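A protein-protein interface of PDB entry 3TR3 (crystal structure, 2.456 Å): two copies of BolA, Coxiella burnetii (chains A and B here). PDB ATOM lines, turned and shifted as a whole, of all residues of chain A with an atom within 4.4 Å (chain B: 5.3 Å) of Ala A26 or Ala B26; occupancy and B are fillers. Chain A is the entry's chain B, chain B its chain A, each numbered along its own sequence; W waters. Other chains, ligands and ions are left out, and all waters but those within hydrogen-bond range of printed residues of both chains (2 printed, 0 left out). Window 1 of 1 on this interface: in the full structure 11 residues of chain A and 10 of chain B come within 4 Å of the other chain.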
ATOM      1  N   THR A   7     -13.945  12.591  23.353  1.00  0.00           N
ATOM      2  CA  THR A   7     -13.166  12.776  22.143  1.00  0.00           C
ATOM      3  C   THR A   7     -13.815  12.083  20.942  1.00  0.00           C
ATOM      4  O   THR A   7     -13.627  12.528  19.817  1.00  0.00           O
ATOM      5  CB  THR A   7     -11.715  12.298  22.298  1.00  0.00           C
ATOM      6  OG1 THR A   7     -11.722  10.902  22.631  1.00  0.00           O
ATOM      7  CG2 THR A   7     -11.013  13.093  23.387  1.00  0.00           C
ATOM      8  N   VAL A  23     -11.050  13.165  11.093  1.00  0.00           N
ATOM      9  CA  VAL A  23     -10.394  13.618  12.331  1.00  0.00           C
ATOM     10  C   VAL A  23      -9.292  12.583  12.768  1.00  0.00           C
ATOM     11  O   VAL A  23      -9.585  11.543  13.379  1.00  0.00           O
ATOM     12  CB  VAL A  23     -11.411  13.949  13.466  1.00  0.00           C
ATOM     13  CG1 VAL A  23     -10.715  14.599  14.655  1.00  0.00           C
ATOM     14  CG2 VAL A  23     -12.526  14.849  12.949  1.00  0.00           C
ATOM     15  N   ILE A  24      -8.042  12.862  12.402  1.00  0.00           N
ATOM     16  CA  ILE A  24      -6.957  11.923  12.617  1.00  0.00           C
ATOM     17  C   ILE A  24      -6.445  11.941  14.070  1.00  0.00           C
ATOM     18  O   ILE A  24      -5.786  11.009  14.518  1.00  0.00           O
ATOM     19  CB  ILE A  24      -5.777  12.108  11.622  1.00  0.00           C
ATOM     20  CG1 ILE A  24      -5.087  13.448  11.841  1.00  0.00           C
ATOM     21  CG2 ILE A  24      -6.227  11.847  10.160  1.00  0.00           C
ATOM     22  CD1 ILE A  24      -3.813  13.552  11.067  1.00  0.00           C
ATOM     23  N   SER A  25      -6.768  12.994  14.802  1.00  0.00           N
ATOM     24  CA  SER A  25      -6.435  13.027  16.193  1.00  0.00           C
ATOM     25  C   SER A  25      -7.416  13.906  16.943  1.00  0.00           C
ATOM     26  O   SER A  25      -7.646  15.028  16.554  1.00  0.00           O
ATOM     27  CB  SER A  25      -5.011  13.520  16.363  1.00  0.00           C
ATOM     28  OG  SER A  25      -4.781  13.920  17.696  1.00  0.00           O
ATOM     29  N   ALA A  26      -8.007  13.371  18.010  1.00  0.00           N
ATOM     30  CA  ALA A  26      -8.865  14.131  18.917  1.00  0.00           C
ATOM     31  C   ALA A  26      -8.466  13.889  20.406  1.00  0.00           C
ATOM     32  O   ALA A  26      -8.485  12.753  20.872  1.00  0.00           O
ATOM     33  CB  ALA A  26     -10.333  13.745  18.678  1.00  0.00           C
ATOM     34  N   GLU A  27      -8.119  14.956  21.131  1.00  0.00           N
ATOM     35  CA  GLU A  27      -7.630  14.872  22.520  1.00  0.00           C
ATOM     36  C   GLU A  27      -8.339  15.882  23.395  1.00  0.00           C
ATOM     37  O   GLU A  27      -8.826  16.903  22.877  1.00  0.00           O
ATOM     38  CB  GLU A  27      -6.101  15.087  22.617  1.00  0.00           C
ATOM     39  CG  GLU A  27      -5.293  14.025  21.870  1.00  0.00           C
ATOM     40  CD  GLU A  27      -3.780  14.298  21.883  1.00  0.00           C
ATOM     41  OE1 GLU A  27      -3.337  15.261  21.180  1.00  0.00           O
ATOM     42  OE2 GLU A  27      -3.044  13.532  22.597  1.00  0.00           O
ATOM     43  N   GLU A  34      -8.341  19.362  21.551  1.00  0.00           N
ATOM     44  CA  GLU A  34      -7.538  19.654  20.362  1.00  0.00           C
ATOM     45  C   GLU A  34      -7.907  18.628  19.326  1.00  0.00           C
ATOM     46  O   GLU A  34      -8.072  17.448  19.638  1.00  0.00           O
ATOM     47  CB  GLU A  34      -6.041  19.517  20.625  1.00  0.00           C
ATOM     48  CG  GLU A  34      -5.493  20.425  21.694  1.00  0.00           C
ATOM     49  CD  GLU A  34      -4.158  19.919  22.239  1.00  0.00           C
ATOM     50  OE1 GLU A  34      -3.814  18.733  21.997  1.00  0.00           O
ATOM     51  OE2 GLU A  34      -3.453  20.710  22.912  1.00  0.00           O
ATOM     52  N   THR B   7      -1.481  11.191  21.495  1.00  0.00           N
ATOM     53  CA  THR B   7      -1.849  10.342  20.356  1.00  0.00           C
ATOM     54  C   THR B   7      -0.728  10.279  19.305  1.00  0.00           C
ATOM     55  O   THR B   7      -0.657   9.346  18.491  1.00  0.00           O
ATOM     56  CB  THR B   7      -3.114  10.880  19.647  1.00  0.00           C
ATOM     57  OG1 THR B   7      -2.911  12.266  19.327  1.00  0.00           O
ATOM     58  CG2 THR B   7      -4.361  10.704  20.516  1.00  0.00           C
ATOM     59  N   VAL B  23      -1.110   3.780  11.746  1.00  0.00           N
ATOM     60  CA  VAL B  23      -2.149   4.305  12.594  1.00  0.00           C
ATOM     61  C   VAL B  23      -2.820   5.489  11.862  1.00  0.00           C
ATOM     62  O   VAL B  23      -2.232   6.549  11.732  1.00  0.00           O
ATOM     63  CB  VAL B  23      -1.593   4.714  13.979  1.00  0.00           C
ATOM     64  CG1 VAL B  23      -2.662   5.366  14.839  1.00  0.00           C
ATOM     65  CG2 VAL B  23      -1.052   3.524  14.674  1.00  0.00           C
ATOM     66  N   ILE B  24      -4.038   5.288  11.368  1.00  0.00           N
ATOM     67  CA  ILE B  24      -4.738   6.331  10.623  1.00  0.00           C
ATOM     68  C   ILE B  24      -5.508   7.306  11.502  1.00  0.00           C
ATOM     69  O   ILE B  24      -5.758   8.436  11.101  1.00  0.00           O
ATOM     70  CB  ILE B  24      -5.716   5.751   9.590  1.00  0.00           C
ATOM     71  CG1 ILE B  24      -6.825   4.993  10.292  1.00  0.00           C
ATOM     72  CG2 ILE B  24      -5.004   4.822   8.660  1.00  0.00           C
ATOM     73  CD1 ILE B  24      -7.799   4.366   9.361  1.00  0.00           C
ATOM     74  N   SER B  25      -5.931   6.880  12.686  1.00  0.00           N
ATOM     75  CA  SER B  25      -6.470   7.864  13.609  1.00  0.00           C
ATOM     76  C   SER B  25      -6.304   7.444  15.047  1.00  0.00           C
ATOM     77  O   SER B  25      -6.066   6.275  15.349  1.00  0.00           O
ATOM     78  CB  SER B  25      -7.941   8.180  13.307  1.00  0.00           C
ATOM     79  OG  SER B  25      -8.779   7.053  13.503  1.00  0.00           O
ATOM     80  N   ALA B  26      -6.458   8.404  15.940  1.00  0.00           N
ATOM     81  CA  ALA B  26      -6.258   8.132  17.333  1.00  0.00           C
ATOM     82  C   ALA B  26      -6.907   9.217  18.164  1.00  0.00           C
ATOM     83  O   ALA B  26      -7.034  10.346  17.731  1.00  0.00           O
ATOM     84  CB  ALA B  26      -4.779   8.013  17.645  1.00  0.00           C
ATOM     85  N   GLU B  27      -7.365   8.819  19.334  1.00  0.00           N
ATOM     86  CA  GLU B  27      -8.007   9.671  20.299  1.00  0.00           C
ATOM     87  C   GLU B  27      -7.289   9.433  21.622  1.00  0.00           C
ATOM     88  O   GLU B  27      -6.709   8.365  21.842  1.00  0.00           O
ATOM     89  CB  GLU B  27      -9.471   9.258  20.443  1.00  0.00           C
ATOM     90  CG  GLU B  27     -10.298   9.395  19.170  1.00  0.00           C
ATOM     91  CD  GLU B  27     -11.616   8.660  19.254  1.00  0.00           C
ATOM     92  OE1 GLU B  27     -12.385   8.965  20.184  1.00  0.00           O
ATOM     93  OE2 GLU B  27     -11.871   7.760  18.411  1.00  0.00           O
ATOM     94  N   GLY B  28      -7.323  10.412  22.506  1.00  0.00           N
ATOM     95  CA  GLY B  28      -6.756  10.214  23.819  1.00  0.00           C
ATOM     96  C   GLY B  28      -7.109  11.311  24.794  1.00  0.00           C
ATOM     97  O   GLY B  28      -7.328  12.433  24.360  1.00  0.00           O
ATOM     98  N   GLU B  34      -7.452   5.547  22.171  1.00  0.00           N
ATOM     99  CA  GLU B  34      -7.929   4.649  21.121  1.00  0.00           C
ATOM    100  C   GLU B  34      -7.087   4.820  19.856  1.00  0.00           C
ATOM    101  O   GLU B  34      -6.614   5.916  19.565  1.00  0.00           O
ATOM    102  CB  GLU B  34      -9.405   4.859  20.825  1.00  0.00           C
ATOM    103  CG  GLU B  34      -9.893   4.068  19.598  1.00  0.00           C
ATOM    104  CD  GLU B  34     -11.369   3.721  19.669  1.00  0.00           C
ATOM    105  OE1 GLU B  34     -11.760   3.034  20.645  1.00  0.00           O
ATOM    106  OE2 GLU B  34     -12.136   4.127  18.761  1.00  0.00           O
ATOM    107  N   ALA B  35      -6.868   3.742  19.118  1.00  0.00           N
ATOM    108  CA  ALA B  35      -6.152   3.840  17.850  1.00  0.00           C
ATOM    109  C   ALA B  35      -6.831   2.980  16.790  1.00  0.00           C
ATOM    110  O   ALA B  35      -7.319   1.890  17.083  1.00  0.00           O
ATOM    111  CB  ALA B  35      -4.686   3.450  18.001  1.00  0.00           C
ATOM    112  N   VAL B  36      -6.888   3.498  15.565  1.00  0.00           N
ATOM    113  CA  VAL B  36      -7.360   2.736  14.412  1.00  0.00           C
ATOM    114  C   VAL B  36      -6.110   2.328  13.657  1.00  0.00           C
ATOM    115  O   VAL B  36      -5.275   3.156  13.332  1.00  0.00           O
ATOM    116  CB  VAL B  36      -8.373   3.558  13.580  1.00  0.00           C
ATOM    117  CG1 VAL B  36      -8.900   2.762  12.379  1.00  0.00           C
ATOM    118  CG2 VAL B  36      -9.527   4.014  14.479  1.00  0.00           C
HETATM  119  O   HOH W   1      -9.653  10.628  16.042  1.00  0.00           O
HETATM  120  O   HOH W   2      -0.667  14.928  19.665  1.00  0.00           O
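The backbone NH (N) of Ala B26 lies within hydrogen-bond range of the backbone carbonyl oxygen (O) of Ile A24 (3.0 Å).
The side-chain hydroxyl (OG) of Ser A25 is in hydrogen-bond range of the side-chain hydroxyl (OG1) of Thr B7 (3.0 Å).
The side-chain carboxylate (OE1) of Glu B27 sits at hydrogen-bond distance from the side-chain hydroxyl (OG1) of Thr A7 (3.2 Å).
N of Gly B28 sits at hydrogen-bond distance from O of Ala A26, 3.1 Å away.
N of Thr B7 lies within hydrogen-bond range of OE2 of Glu A27 (3.0 Å).
The backbone NH (N) of Ala A26 sits at hydrogen-bond distance from the backbone carbonyl oxygen (O) of Ala B26.
The backbone carbonyl oxygen (O) of Glu B27 lies within hydrogen-bond range of the backbone NH (N) of Glu B34, at 2.9 Å.
N of Glu A34 is in hydrogen-bond range of O of Glu A27 (2.8 Å).
The backbone carbonyl oxygen of Ser B25 lies within hydrogen-bond range of the backbone NH of Val B36, at 2.9 Å.
The backbone carbonyl oxygen (O) of Val B36 sits at hydrogen-bond distance from the backbone NH (N) of Ile B24 (3.2 Å).
Thr A7 touches Gly B28 (CG2 to O, 3.9 Å).
Val A23 touches Ser B25 (O to CB, 3.7 Å).
Ile A24 touches Ile B24.
Ser B25 touches Ile A24 (CA to O, 3.3 Å).
Ser A25 touches Ala B26.
Glu B27 touches Ala A26 (CA to O, 3.2 Å).
Glu A27 touches Gly B28.
Of the printed residues of chain B, Ala A26 touches Ala B26, Glu B27 and Gly B28.
Of chain A, only Ile A24, Ser A25 and Ala A26 come within 4 Å of Ala B26.
Of the printed residues of chain A, Ser B25 touches Val A23 and Ile A24.
Of the printed residues of chain B, Val A23 touches Ser B25 (3.7 Å).
The nearest residue of chain B that does not touch Ala A26 is Thr B7 (4.6 Å).
The nearest printed residue of chain A that does not touch Ala B26 is Val A23 (5.1 Å).
Along chain B the printed residues that touch a printed residue of chain A span positions 7 to 28.
Hydrophobic or aromatic side chains of chain A that line the printed part of chain B: Ile A24.
Along chain A the printed residues that touch a printed residue of chain B span positions 7 to 27.
Thr A7 touches Glu B27, and with the chains exchanged Glu A27 touches Thr B7.
Val A23 touches Ser B25, but with the chains exchanged Ser A25 does not touch Val B23 (8.5 Å).
Ser A25 touches Thr B7, but with the chains exchanged Thr A7 does not touch Ser B25 (9.7 Å).
Ala A26 touches its own counterpart, Ala B26.
Positions printed for both chains: 7, 23, 24, 25, 26, 27 and 34.
Of the 13 pairs that touch across the chains among the printed residues, 4 have their exchanged pair printed and touching as well.
Water W1 bridges O of Val A23 (2.8 Å) and O of Ala B26 (3.1 Å).
Water W2 bridges the side-chain carboxylate (OE1) of Glu A27 and the side-chain hydroxyl (OG1) of Thr B7.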
